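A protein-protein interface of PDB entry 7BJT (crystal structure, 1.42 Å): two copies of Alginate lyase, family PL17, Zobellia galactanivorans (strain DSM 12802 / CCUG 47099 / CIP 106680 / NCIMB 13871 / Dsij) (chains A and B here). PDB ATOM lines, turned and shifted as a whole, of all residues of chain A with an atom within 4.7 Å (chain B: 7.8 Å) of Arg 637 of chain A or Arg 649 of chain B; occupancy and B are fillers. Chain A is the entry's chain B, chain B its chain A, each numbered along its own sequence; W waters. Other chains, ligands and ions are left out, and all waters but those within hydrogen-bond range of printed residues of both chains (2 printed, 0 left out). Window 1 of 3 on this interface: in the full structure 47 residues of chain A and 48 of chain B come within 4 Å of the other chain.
The guanidinium group (NH1) of Arg 637 of chain B lies within hydrogen-bond range of the backbone carbonyl oxygen (O) of Arg 649 of chain B (3.0 Å).
The guanidinium group of Arg 649 of chain B lies within hydrogen-bond range of the backbone carbonyl oxygen of Gly 639 of chain B (3.2 Å).
The backbone carbonyl oxygen (O) of Leu 647 of chain B is in hydrogen-bond range of the guanidinium group (NH1) of Arg 649 of chain B (2.9 Å).
The backbone carbonyl oxygen (O) of Arg 637 of chain A is in hydrogen-bond range of the backbone NH (N) of Trp 598 of chain A, at 2.8 Å.
The side-chain carboxylate of Glu 600 of chain A lies within salt-bridge range of the guanidinium group of Arg 637 of chain A, at 2.8 Å.
O of Gly 639 of chain A sits at hydrogen-bond distance from NH2 of Arg 649 of chain A, 3.3 Å away.
Along chain B the printed residues that touch a printed residue of chain A span positions 585 to 649.
Of the 12 printed residues of chain A, 5 touch a printed residue of chain B.
Hydrophobic or aromatic side chains of chain A that line the printed part of chain B: Trp 598 and Phe 635.
Glu 600 of chain A touches Arg 649 of chain B, and with the chains exchanged Arg 649 of chain A touches Glu 600 of chain B.
Arg 637 of chain A touches Arg 649 of chain B, and with the chains exchanged Arg 649 of chain A touches Arg 637 of chain B.
10 positions are printed for both chains.
Among the printed residues, pairs that only touch across the chains: Trp 598 of chain A with Leu 585 of chain B, Arg 649 of chain A with Arg 637 of chain B, Arg 637 of chain A with Arg 649 of chain B, Glu 600 of chain A with Phe 645 of chain B and Phe 635 of chain A with Phe 645 of chain B.
Of the printed residues of chain B, Glu 600 of chain A touches Phe 645 and Arg 649.
Of the printed residues of chain B, Phe 635 of chain A touches Phe 645 (3.8 Å).
Of chain B, only Arg 649 comes within 4 Å of Arg 637 of chain A.
Printed residues of chain B within 4 Å of Arg 649 of chain A: Glu 600 (2.8 Å) and Arg 637 (3.5 Å).
Printed residues of chain A within 4 Å of Leu 585 of chain B: Trp 598.
Arg 649 of chain B touches just these residues of chain A: Glu 600 and Arg 637.
The nearest residue of chain B that does not touch Arg 637 of chain A is Phe 645 of chain B (4.3 Å).
The nearest printed residue of chain A that does not touch Arg 649 of chain B is Arg 649 of chain A (5.2 Å).
The side-chain carboxylate (OE2) of Glu 600 of chain B is in salt-bridge range of the guanidinium group (NH2) of Arg 649 of chain A.
NE of Arg 649 of chain B is in salt-bridge range of OE2 of Glu 600 of chain A (3.8 Å).
Water W2 lies within hydrogen-bond range of OE2 of Glu 600 of chain B (2.5 Å), NE1 of Trp 598 of chain A (2.8 Å), NH2 of Arg 649 of chain A (3.2 Å) and O of Gly 639 of chain A (3.3 Å).
Water W1 lies within hydrogen-bond range of the indole nitrogen of Trp 598 of chain B (2.8 Å), the side-chain carboxylate of Glu 600 of chain A (2.9 Å), the guanidinium group of Arg 649 of chain B (3.1 Å) and the backbone carbonyl oxygen of Gly 639 of chain B (3.4 Å).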
ATOM      1  N   HIS A 596      28.252   3.683  15.944  1.00  0.00           N
ATOM      2  CA  HIS A 596      27.498   2.613  16.594  1.00  0.00           C
ATOM      3  C   HIS A 596      27.063   1.504  15.643  1.00  0.00           C
ATOM      4  O   HIS A 596      26.411   0.552  16.085  1.00  0.00           O
ATOM      5  CB  HIS A 596      26.283   3.186  17.323  1.00  0.00           C
ATOM      6  CG  HIS A 596      26.634   4.114  18.443  1.00  0.00           C
ATOM      7  ND1 HIS A 596      27.391   3.720  19.526  1.00  0.00           N
ATOM      8  CD2 HIS A 596      26.321   5.415  18.654  1.00  0.00           C
ATOM      9  CE1 HIS A 596      27.527   4.739  20.357  1.00  0.00           C
ATOM     10  NE2 HIS A 596      26.885   5.776  19.855  1.00  0.00           N
ATOM     11  N   LEU A 597      27.434   1.594  14.366  1.00  0.00           N
ATOM     12  CA  LEU A 597      27.066   0.561  13.386  1.00  0.00           C
ATOM     13  C   LEU A 597      28.272  -0.259  12.977  1.00  0.00           C
ATOM     14  O   LEU A 597      29.271   0.300  12.548  1.00  0.00           O
ATOM     15  CB  LEU A 597      26.456   1.199  12.136  1.00  0.00           C
ATOM     16  CG  LEU A 597      25.069   1.813  12.319  1.00  0.00           C
ATOM     17  CD1 LEU A 597      24.682   2.599  11.080  1.00  0.00           C
ATOM     18  CD2 LEU A 597      24.030   0.740  12.622  1.00  0.00           C
ATOM     19  N   TRP A 598      28.170  -1.581  13.113  1.00  0.00           N
ATOM     20  CA  TRP A 598      29.147  -2.494  12.524  1.00  0.00           C
ATOM     21  C   TRP A 598      28.793  -2.712  11.060  1.00  0.00           C
ATOM     22  O   TRP A 598      27.621  -2.886  10.726  1.00  0.00           O
ATOM     23  CB  TRP A 598      29.108  -3.869  13.193  1.00  0.00           C
ATOM     24  CG  TRP A 598      29.480  -3.926  14.634  1.00  0.00           C
ATOM     25  CD1 TRP A 598      28.681  -4.337  15.678  1.00  0.00           C
ATOM     26  CD2 TRP A 598      30.744  -3.615  15.197  1.00  0.00           C
ATOM     27  NE1 TRP A 598      29.377  -4.284  16.846  1.00  0.00           N
ATOM     28  CE2 TRP A 598      30.647  -3.838  16.589  1.00  0.00           C
ATOM     29  CE3 TRP A 598      31.950  -3.151  14.670  1.00  0.00           C
ATOM     30  CZ2 TRP A 598      31.714  -3.617  17.460  1.00  0.00           C
ATOM     31  CZ3 TRP A 598      33.027  -2.931  15.546  1.00  0.00           C
ATOM     32  CH2 TRP A 598      32.897  -3.166  16.920  1.00  0.00           C
ATOM     33  N   GLU A 600      28.516  -5.205   8.480  1.00  0.00           N
ATOM     34  CA  GLU A 600      28.394  -6.669   8.422  1.00  0.00           C
ATOM     35  C   GLU A 600      28.490  -7.244   7.018  1.00  0.00           C
ATOM     36  O   GLU A 600      28.778  -8.430   6.855  1.00  0.00           O
ATOM     37  CB  GLU A 600      27.083  -7.122   9.059  1.00  0.00           C
ATOM     38  CG  GLU A 600      27.087  -7.049  10.569  1.00  0.00           C
ATOM     39  CD  GLU A 600      26.083  -7.991  11.199  1.00  0.00           C
ATOM     40  OE1 GLU A 600      24.986  -8.183  10.641  1.00  0.00           O
ATOM     41  OE2 GLU A 600      26.368  -8.515  12.300  1.00  0.00           O
ATOM     42  N   PHE A 635      24.911  -3.943   4.671  1.00  0.00           N
ATOM     43  CA  PHE A 635      24.308  -4.631   5.807  1.00  0.00           C
ATOM     44  C   PHE A 635      25.009  -4.121   7.054  1.00  0.00           C
ATOM     45  O   PHE A 635      26.231  -4.220   7.156  1.00  0.00           O
ATOM     46  CB  PHE A 635      24.487  -6.139   5.710  1.00  0.00           C
ATOM     47  CG  PHE A 635      23.518  -6.817   4.787  1.00  0.00           C
ATOM     48  CD1 PHE A 635      22.190  -6.987   5.161  1.00  0.00           C
ATOM     49  CD2 PHE A 635      23.941  -7.325   3.564  1.00  0.00           C
ATOM     50  CE1 PHE A 635      21.298  -7.648   4.329  1.00  0.00           C
ATOM     51  CE2 PHE A 635      23.053  -7.983   2.732  1.00  0.00           C
ATOM     52  CZ  PHE A 635      21.732  -8.134   3.113  1.00  0.00           C
ATOM     53  N   VAL A 636      24.228  -3.600   7.996  1.00  0.00           N
ATOM     54  CA  VAL A 636      24.772  -3.044   9.233  1.00  0.00           C
ATOM     55  C   VAL A 636      24.155  -3.705  10.442  1.00  0.00           C
ATOM     56  O   VAL A 636      23.085  -4.302  10.353  1.00  0.00           O
ATOM     57  CB  VAL A 636      24.610  -1.509   9.323  1.00  0.00           C
ATOM     58  CG1 VAL A 636      25.362  -0.834   8.183  1.00  0.00           C
ATOM     59  CG2 VAL A 636      23.150  -1.068   9.343  1.00  0.00           C
ATOM     60  N   ARG A 637      24.851  -3.602  11.572  1.00  0.00           N
ATOM     61  CA  ARG A 637      24.292  -4.047  12.830  1.00  0.00           C
ATOM     62  C   ARG A 637      24.633  -3.061  13.925  1.00  0.00           C
ATOM     63  O   ARG A 637      25.780  -2.652  14.078  1.00  0.00           O
ATOM     64  CB  ARG A 637      24.765  -5.444  13.213  1.00  0.00           C
ATOM     65  CG  ARG A 637      23.941  -5.994  14.383  1.00  0.00           C
ATOM     66  CD  ARG A 637      24.104  -7.452  14.630  1.00  0.00           C
ATOM     67  NE  ARG A 637      23.788  -8.202  13.432  1.00  0.00           N
ATOM     68  CZ  ARG A 637      22.585  -8.666  13.091  1.00  0.00           C
ATOM     69  NH1 ARG A 637      21.504  -8.494  13.845  1.00  0.00           N
ATOM     70  NH2 ARG A 637      22.488  -9.346  11.955  1.00  0.00           N
ATOM     71  N   ILE A 638      23.620  -2.717  14.704  1.00  0.00           N
ATOM     72  CA  ILE A 638      23.795  -1.792  15.808  1.00  0.00           C
ATOM     73  C   ILE A 638      24.593  -2.500  16.899  1.00  0.00           C
ATOM     74  O   ILE A 638      24.424  -3.698  17.127  1.00  0.00           O
ATOM     75  CB  ILE A 638      22.435  -1.331  16.362  1.00  0.00           C
ATOM     76  CG1 ILE A 638      21.602  -0.653  15.263  1.00  0.00           C
ATOM     77  CG2 ILE A 638      22.625  -0.391  17.549  1.00  0.00           C
ATOM     78  CD1 ILE A 638      20.156  -0.425  15.643  1.00  0.00           C
ATOM     79  N   GLY A 639      25.474  -1.756  17.558  1.00  0.00           N
ATOM     80  CA  GLY A 639      26.196  -2.262  18.717  1.00  0.00           C
ATOM     81  C   GLY A 639      27.654  -1.892  18.848  1.00  0.00           C
ATOM     82  O   GLY A 639      28.265  -2.230  19.856  1.00  0.00           O
ATOM     83  N   ARG A 649      21.071  -5.215  19.306  1.00  0.00           N
ATOM     84  CA  ARG A 649      21.802  -5.683  18.118  1.00  0.00           C
ATOM     85  C   ARG A 649      20.858  -5.900  16.923  1.00  0.00           C
ATOM     86  O   ARG A 649      20.878  -6.957  16.272  1.00  0.00           O
ATOM     87  CB  ARG A 649      22.631  -6.948  18.440  1.00  0.00           C
ATOM     88  CG  ARG A 649      24.078  -6.679  18.818  1.00  0.00           C
ATOM     89  CD  ARG A 649      24.186  -5.812  20.042  1.00  0.00           C
ATOM     90  NE  ARG A 649      25.568  -5.642  20.513  1.00  0.00           N
ATOM     91  CZ  ARG A 649      25.948  -4.730  21.408  1.00  0.00           C
ATOM     92  NH1 ARG A 649      25.065  -3.907  21.939  1.00  0.00           N
ATOM     93  NH2 ARG A 649      27.226  -4.640  21.773  1.00  0.00           N
ATOM     94  N   ASP A 650      20.067  -4.882  16.607  1.00  0.00           N
ATOM     95  CA  ASP A 650      19.195  -4.914  15.432  1.00  0.00           C
ATOM     96  C   ASP A 650      20.018  -4.630  14.174  1.00  0.00           C
ATOM     97  O   ASP A 650      21.103  -4.045  14.244  1.00  0.00           O
ATOM     98  CB  ASP A 650      18.076  -3.873  15.564  1.00  0.00           C
ATOM     99  CG  ASP A 650      17.187  -4.088  16.794  1.00  0.00           C
ATOM    100  OD1 ASP A 650      16.901  -5.250  17.150  1.00  0.00           O
ATOM    101  OD2 ASP A 650      16.722  -3.067  17.366  1.00  0.00           O
ATOM    102  N   ALA A 651      19.489  -5.047  13.030  1.00  0.00           N
ATOM    103  CA  ALA A 651      20.171  -4.934  11.741  1.00  0.00           C
ATOM    104  C   ALA A 651      19.532  -3.885  10.843  1.00  0.00           C
ATOM    105  O   ALA A 651      18.416  -3.424  11.075  1.00  0.00           O
ATOM    106  CB  ALA A 651      20.159  -6.281  11.036  1.00  0.00           C
ATOM    107  N   GLN B 448      19.945 -21.433  26.212  1.00  0.00           N
ATOM    108  CA  GLN B 448      19.511 -22.208  25.045  1.00  0.00           C
ATOM    109  C   GLN B 448      20.426 -23.348  24.653  1.00  0.00           C
ATOM    110  O   GLN B 448      21.638 -23.299  24.868  1.00  0.00           O
ATOM    111  CB  GLN B 448      19.314 -21.312  23.814  1.00  0.00           C
ATOM    112  CG  GLN B 448      20.578 -20.703  23.228  1.00  0.00           C
ATOM    113  CD  GLN B 448      20.383 -20.143  21.840  1.00  0.00           C
ATOM    114  OE1 GLN B 448      19.739 -20.761  20.987  1.00  0.00           O
ATOM    115  NE2 GLN B 448      20.978 -18.989  21.583  1.00  0.00           N
ATOM    116  N   TYR B 450      21.122 -24.465  20.927  1.00  0.00           N
ATOM    117  CA  TYR B 450      20.937 -23.722  19.676  1.00  0.00           C
ATOM    118  C   TYR B 450      19.915 -24.362  18.743  1.00  0.00           C
ATOM    119  O   TYR B 450      19.172 -23.647  18.075  1.00  0.00           O
ATOM    120  CB  TYR B 450      22.268 -23.502  18.926  1.00  0.00           C
ATOM    121  CG  TYR B 450      22.114 -22.542  17.760  1.00  0.00           C
ATOM    122  CD1 TYR B 450      21.756 -23.002  16.499  1.00  0.00           C
ATOM    123  CD2 TYR B 450      22.286 -21.179  17.931  1.00  0.00           C
ATOM    124  CE1 TYR B 450      21.573 -22.128  15.439  1.00  0.00           C
ATOM    125  CE2 TYR B 450      22.123 -20.298  16.875  1.00  0.00           C
ATOM    126  CZ  TYR B 450      21.746 -20.773  15.631  1.00  0.00           C
ATOM    127  OH  TYR B 450      21.540 -19.906  14.570  1.00  0.00           O
ATOM    128  N   LEU B 585      35.421  -6.205  15.849  1.00  0.00           N
ATOM    129  CA  LEU B 585      35.083  -7.556  16.303  1.00  0.00           C
ATOM    130  C   LEU B 585      35.881  -8.563  15.503  1.00  0.00           C
ATOM    131  O   LEU B 585      35.873  -8.539  14.277  1.00  0.00           O
ATOM    132  CB  LEU B 585      33.584  -7.842  16.218  1.00  0.00           C
ATOM    133  CG  LEU B 585      32.714  -6.832  16.991  1.00  0.00           C
ATOM    134  CD1 LEU B 585      31.228  -7.152  16.880  1.00  0.00           C
ATOM    135  CD2 LEU B 585      33.122  -6.726  18.457  1.00  0.00           C
ATOM    136  N   HIS B 596      32.746 -19.031  14.294  1.00  0.00           N
ATOM    137  CA  HIS B 596      31.431 -18.400  14.180  1.00  0.00           C
ATOM    138  C   HIS B 596      31.097 -17.463  15.334  1.00  0.00           C
ATOM    139  O   HIS B 596      30.008 -16.895  15.357  1.00  0.00           O
ATOM    140  CB  HIS B 596      30.338 -19.467  14.044  1.00  0.00           C
ATOM    141  CG  HIS B 596      30.454 -20.298  12.804  1.00  0.00           C
ATOM    142  ND1 HIS B 596      30.385 -19.762  11.537  1.00  0.00           N
ATOM    143  CD2 HIS B 596      30.595 -21.634  12.639  1.00  0.00           C
ATOM    144  CE1 HIS B 596      30.478 -20.733  10.644  1.00  0.00           C
ATOM    145  NE2 HIS B 596      30.612 -21.877  11.287  1.00  0.00           N
ATOM    146  N   TRP B 598      31.966 -13.967  17.344  1.00  0.00           N
ATOM    147  CA  TRP B 598      32.661 -12.695  17.490  1.00  0.00           C
ATOM    148  C   TRP B 598      32.995 -12.489  18.965  1.00  0.00           C
ATOM    149  O   TRP B 598      32.158 -12.748  19.826  1.00  0.00           O
ATOM    150  CB  TRP B 598      31.770 -11.527  17.059  1.00  0.00           C
ATOM    151  CG  TRP B 598      31.374 -11.484  15.630  1.00  0.00           C
ATOM    152  CD1 TRP B 598      30.094 -11.545  15.117  1.00  0.00           C
ATOM    153  CD2 TRP B 598      32.237 -11.319  14.521  1.00  0.00           C
ATOM    154  NE1 TRP B 598      30.128 -11.441  13.762  1.00  0.00           N
ATOM    155  CE2 TRP B 598      31.429 -11.303  13.359  1.00  0.00           C
ATOM    156  CE3 TRP B 598      33.620 -11.200  14.384  1.00  0.00           C
ATOM    157  CZ2 TRP B 598      31.962 -11.164  12.079  1.00  0.00           C
ATOM    158  CZ3 TRP B 598      34.155 -11.059  13.104  1.00  0.00           C
ATOM    159  CH2 TRP B 598      33.327 -11.051  11.972  1.00  0.00           C
ATOM    160  N   GLU B 600      33.060 -10.051  21.622  1.00  0.00           N
ATOM    161  CA  GLU B 600      32.405  -8.759  21.860  1.00  0.00           C
ATOM    162  C   GLU B 600      32.922  -8.032  23.106  1.00  0.00           C
ATOM    163  O   GLU B 600      32.801  -6.814  23.206  1.00  0.00           O
ATOM    164  CB  GLU B 600      30.882  -8.943  21.943  1.00  0.00           C
ATOM    165  CG  GLU B 600      30.090  -7.711  21.534  1.00  0.00           C
ATOM    166  CD  GLU B 600      28.616  -7.963  21.259  1.00  0.00           C
ATOM    167  OE1 GLU B 600      28.072  -8.998  21.646  1.00  0.00           O
ATOM    168  OE2 GLU B 600      27.971  -7.075  20.664  1.00  0.00           O
ATOM    169  N   VAL B 636      30.487 -13.117  23.879  1.00  0.00           N
ATOM    170  CA  VAL B 636      30.544 -13.534  22.480  1.00  0.00           C
ATOM    171  C   VAL B 636      29.214 -13.289  21.783  1.00  0.00           C
ATOM    172  O   VAL B 636      28.179 -13.130  22.426  1.00  0.00           O
ATOM    173  CB  VAL B 636      30.975 -15.017  22.338  1.00  0.00           C
ATOM    174  CG1 VAL B 636      32.357 -15.215  22.944  1.00  0.00           C
ATOM    175  CG2 VAL B 636      29.971 -15.977  22.976  1.00  0.00           C
ATOM    176  N   ARG B 637      29.269 -13.256  20.457  1.00  0.00           N
ATOM    177  CA  ARG B 637      28.083 -13.067  19.620  1.00  0.00           C
ATOM    178  C   ARG B 637      28.207 -14.026  18.447  1.00  0.00           C
ATOM    179  O   ARG B 637      29.216 -14.021  17.755  1.00  0.00           O
ATOM    180  CB  ARG B 637      28.060 -11.619  19.135  1.00  0.00           C
ATOM    181  CG  ARG B 637      27.004 -11.209  18.115  1.00  0.00           C
ATOM    182  CD  ARG B 637      25.679 -10.797  18.708  1.00  0.00           C
ATOM    183  NE  ARG B 637      25.799  -9.912  19.873  1.00  0.00           N
ATOM    184  CZ  ARG B 637      24.818  -9.675  20.742  1.00  0.00           C
ATOM    185  NH1 ARG B 637      23.621 -10.227  20.589  1.00  0.00           N
ATOM    186  NH2 ARG B 637      25.054  -8.889  21.788  1.00  0.00           N
ATOM    187  N   ILE B 638      27.181 -14.838  18.220  1.00  0.00           N
ATOM    188  CA  ILE B 638      27.170 -15.742  17.077  1.00  0.00           C
ATOM    189  C   ILE B 638      27.005 -14.896  15.814  1.00  0.00           C
ATOM    190  O   ILE B 638      26.287 -13.902  15.820  1.00  0.00           O
ATOM    191  CB  ILE B 638      26.026 -16.767  17.190  1.00  0.00           C
ATOM    192  CG1 ILE B 638      26.142 -17.581  18.489  1.00  0.00           C
ATOM    193  CG2 ILE B 638      25.996 -17.700  15.974  1.00  0.00           C
ATOM    194  CD1 ILE B 638      24.925 -18.444  18.783  1.00  0.00           C
ATOM    195  N   GLY B 639      27.687 -15.288  14.742  1.00  0.00           N
ATOM    196  CA  GLY B 639      27.507 -14.667  13.428  1.00  0.00           C
ATOM    197  C   GLY B 639      28.747 -14.456  12.589  1.00  0.00           C
ATOM    198  O   GLY B 639      28.620 -14.032  11.447  1.00  0.00           O
ATOM    199  N   ALA B 640      29.942 -14.733  13.120  1.00  0.00           N
ATOM    200  CA  ALA B 640      31.147 -14.680  12.303  1.00  0.00           C
ATOM    201  C   ALA B 640      31.136 -15.805  11.270  1.00  0.00           C
ATOM    202  O   ALA B 640      30.494 -16.843  11.471  1.00  0.00           O
ATOM    203  CB  ALA B 640      32.400 -14.758  13.174  1.00  0.00           C
ATOM    204  N   ASN B 641      31.834 -15.582  10.156  1.00  0.00           N
ATOM    205  CA  ASN B 641      31.921 -16.561   9.075  1.00  0.00           C
ATOM    206  C   ASN B 641      30.541 -17.120   8.701  1.00  0.00           C
ATOM    207  O   ASN B 641      30.338 -18.324   8.640  1.00  0.00           O
ATOM    208  CB  ASN B 641      32.921 -17.664   9.443  1.00  0.00           C
ATOM    209  CG  ASN B 641      34.355 -17.174   9.390  1.00  0.00           C
ATOM    210  OD1 ASN B 641      35.026 -17.024  10.414  1.00  0.00           O
ATOM    211  ND2 ASN B 641      34.820 -16.882   8.186  1.00  0.00           N
ATOM    212  N   ASP B 642      29.599 -16.212   8.462  1.00  0.00           N
ATOM    213  CA  ASP B 642      28.207 -16.562   8.160  1.00  0.00           C
ATOM    214  C   ASP B 642      27.756 -15.766   6.935  1.00  0.00           C
ATOM    215  O   ASP B 642      26.883 -14.897   7.033  1.00  0.00           O
ATOM    216  CB  ASP B 642      27.317 -16.278   9.380  1.00  0.00           C
ATOM    217  CG  ASP B 642      25.866 -16.674   9.166  1.00  0.00           C
ATOM    218  OD1 ASP B 642      25.591 -17.604   8.381  1.00  0.00           O
ATOM    219  OD2 ASP B 642      24.993 -16.052   9.789  1.00  0.00           O
ATOM    220  N   PRO B 643      28.352 -16.067   5.769  1.00  0.00           N
ATOM    221  CA  PRO B 643      28.137 -15.237   4.584  1.00  0.00           C
ATOM    222  C   PRO B 643      26.701 -15.172   4.050  1.00  0.00           C
ATOM    223  O   PRO B 643      26.375 -14.234   3.321  1.00  0.00           O
ATOM    224  CB  PRO B 643      29.089 -15.856   3.549  1.00  0.00           C
ATOM    225  CG  PRO B 643      29.293 -17.253   3.999  1.00  0.00           C
ATOM    226  CD  PRO B 643      29.308 -17.153   5.496  1.00  0.00           C
ATOM    227  N   GLU B 644      25.852 -16.134   4.409  1.00  0.00           N
ATOM    228  CA  GLU B 644      24.464 -16.165   3.944  1.00  0.00           C
ATOM    229  C   GLU B 644      23.447 -15.765   5.020  1.00  0.00           C
ATOM    230  O   GLU B 644      22.243 -15.906   4.799  1.00  0.00           O
ATOM    231  CB  GLU B 644      24.139 -17.565   3.413  1.00  0.00           C
ATOM    232  CG  GLU B 644      25.068 -18.006   2.293  1.00  0.00           C
ATOM    233  CD  GLU B 644      24.693 -19.357   1.729  1.00  0.00           C
ATOM    234  OE1 GLU B 644      24.613 -20.328   2.512  1.00  0.00           O
ATOM    235  OE2 GLU B 644      24.469 -19.452   0.500  1.00  0.00           O
ATOM    236  N   PHE B 645      23.910 -15.246   6.162  1.00  0.00           N
ATOM    237  CA  PHE B 645      23.020 -14.940   7.301  1.00  0.00           C
ATOM    238  C   PHE B 645      22.173 -16.170   7.677  1.00  0.00           C
ATOM    239  O   PHE B 645      20.942 -16.101   7.790  1.00  0.00           O
ATOM    240  CB  PHE B 645      22.127 -13.717   7.018  1.00  0.00           C
ATOM    241  CG  PHE B 645      22.870 -12.406   6.969  1.00  0.00           C
ATOM    242  CD1 PHE B 645      23.341 -11.815   8.137  1.00  0.00           C
ATOM    243  CD2 PHE B 645      23.079 -11.739   5.762  1.00  0.00           C
ATOM    244  CE1 PHE B 645      24.011 -10.601   8.106  1.00  0.00           C
ATOM    245  CE2 PHE B 645      23.748 -10.525   5.729  1.00  0.00           C
ATOM    246  CZ  PHE B 645      24.216  -9.960   6.901  1.00  0.00           C
ATOM    247  N   ASN B 646      22.847 -17.305   7.844  1.00  0.00           N
ATOM    248  CA  ASN B 646      22.193 -18.538   8.275  1.00  0.00           C
ATOM    249  C   ASN B 646      22.109 -18.729   9.782  1.00  0.00           C
ATOM    250  O   ASN B 646      21.387 -19.635  10.237  1.00  0.00           O
ATOM    251  CB  ASN B 646      22.896 -19.753   7.664  1.00  0.00           C
ATOM    252  CG  ASN B 646      22.710 -19.851   6.165  1.00  0.00           C
ATOM    253  OD1 ASN B 646      21.781 -19.279   5.598  1.00  0.00           O
ATOM    254  ND2 ASN B 646      23.580 -20.620   5.517  1.00  0.00           N
ATOM    255  N   LEU B 647      22.835 -17.905  10.544  1.00  0.00           N
ATOM    256  CA  LEU B 647      22.895 -18.019  12.004  1.00  0.00           C
ATOM    257  C   LEU B 647      22.273 -16.816  12.697  1.00  0.00           C
ATOM    258  O   LEU B 647      22.349 -15.691  12.204  1.00  0.00           O
ATOM    259  CB  LEU B 647      24.348 -18.164  12.466  1.00  0.00           C
ATOM    260  CG  LEU B 647      25.098 -19.401  11.948  1.00  0.00           C
ATOM    261  CD1 LEU B 647      26.554 -19.403  12.402  1.00  0.00           C
ATOM    262  CD2 LEU B 647      24.402 -20.684  12.381  1.00  0.00           C
ATOM    263  N   ARG B 648      21.681 -17.065  13.862  1.00  0.00           N
ATOM    264  CA  ARG B 648      21.118 -16.003  14.697  1.00  0.00           C
ATOM    265  C   ARG B 648      22.210 -15.277  15.451  1.00  0.00           C
ATOM    266  O   ARG B 648      23.148 -15.920  15.945  1.00  0.00           O
ATOM    267  CB  ARG B 648      20.155 -16.583  15.731  1.00  0.00           C
ATOM    268  CG  ARG B 648      18.958 -17.294  15.145  1.00  0.00           C
ATOM    269  CD  ARG B 648      17.966 -17.680  16.227  1.00  0.00           C
ATOM    270  NE  ARG B 648      18.517 -18.612  17.217  1.00  0.00           N
ATOM    271  CZ  ARG B 648      18.549 -19.937  17.084  1.00  0.00           C
ATOM    272  NH1 ARG B 648      18.095 -20.534  15.982  1.00  0.00           N
ATOM    273  NH2 ARG B 648      19.031 -20.685  18.067  1.00  0.00           N
ATOM    274  N   ARG B 649      22.036 -13.971  15.638  1.00  0.00           N
ATOM    275  CA  ARG B 649      22.996 -13.145  16.387  1.00  0.00           C
ATOM    276  C   ARG B 649      22.728 -13.182  17.897  1.00  0.00           C
ATOM    277  O   ARG B 649      22.628 -12.147  18.559  1.00  0.00           O
ATOM    278  CB  ARG B 649      23.023 -11.703  15.835  1.00  0.00           C
ATOM    279  CG  ARG B 649      24.119 -11.437  14.818  1.00  0.00           C
ATOM    280  CD  ARG B 649      23.932 -12.287  13.589  1.00  0.00           C
ATOM    281  NE  ARG B 649      24.881 -11.954  12.522  1.00  0.00           N
ATOM    282  CZ  ARG B 649      25.132 -12.733  11.476  1.00  0.00           C
ATOM    283  NH1 ARG B 649      24.501 -13.892  11.318  1.00  0.00           N
ATOM    284  NH2 ARG B 649      26.017 -12.344  10.566  1.00  0.00           N
ATOM    285  N   ASP B 650      22.641 -14.391  18.445  1.00  0.00           N
ATOM    286  CA  ASP B 650      22.472 -14.594  19.887  1.00  0.00           C
ATOM    287  C   ASP B 650      23.815 -14.411  20.588  1.00  0.00           C
ATOM    288  O   ASP B 650      24.877 -14.567  19.968  1.00  0.00           O
ATOM    289  CB  ASP B 650      21.932 -15.993  20.182  1.00  0.00           C
ATOM    290  CG  ASP B 650      20.566 -16.265  19.558  1.00  0.00           C
ATOM    291  OD1 ASP B 650      19.740 -15.341  19.491  1.00  0.00           O
ATOM    292  OD2 ASP B 650      20.323 -17.435  19.166  1.00  0.00           O
ATOM    293  N   ALA B 651      23.765 -14.095  21.880  1.00  0.00           N
ATOM    294  CA  ALA B 651      24.966 -13.811  22.679  1.00  0.00           C
ATOM    295  C   ALA B 651      25.297 -14.946  23.639  1.00  0.00           C
ATOM    296  O   ALA B 651      24.488 -15.840  23.887  1.00  0.00           O
ATOM    297  CB  ALA B 651      24.776 -12.522  23.457  1.00  0.00           C
ATOM    298  N   GLY B 652      26.500 -14.901  24.199  1.00  0.00           N
ATOM    299  CA  GLY B 652      26.872 -15.811  25.277  1.00  0.00           C
ATOM    300  C   GLY B 652      27.943 -15.219  26.167  1.00  0.00           C
ATOM    301  O   GLY B 652      28.608 -14.248  25.791  1.00  0.00           O
HETATM  302  O   HOH W   1      28.267 -10.649  11.764  1.00  0.00           O
HETATM  303  O   HOH W   2      29.309  -5.304  19.413  1.00  0.00           O
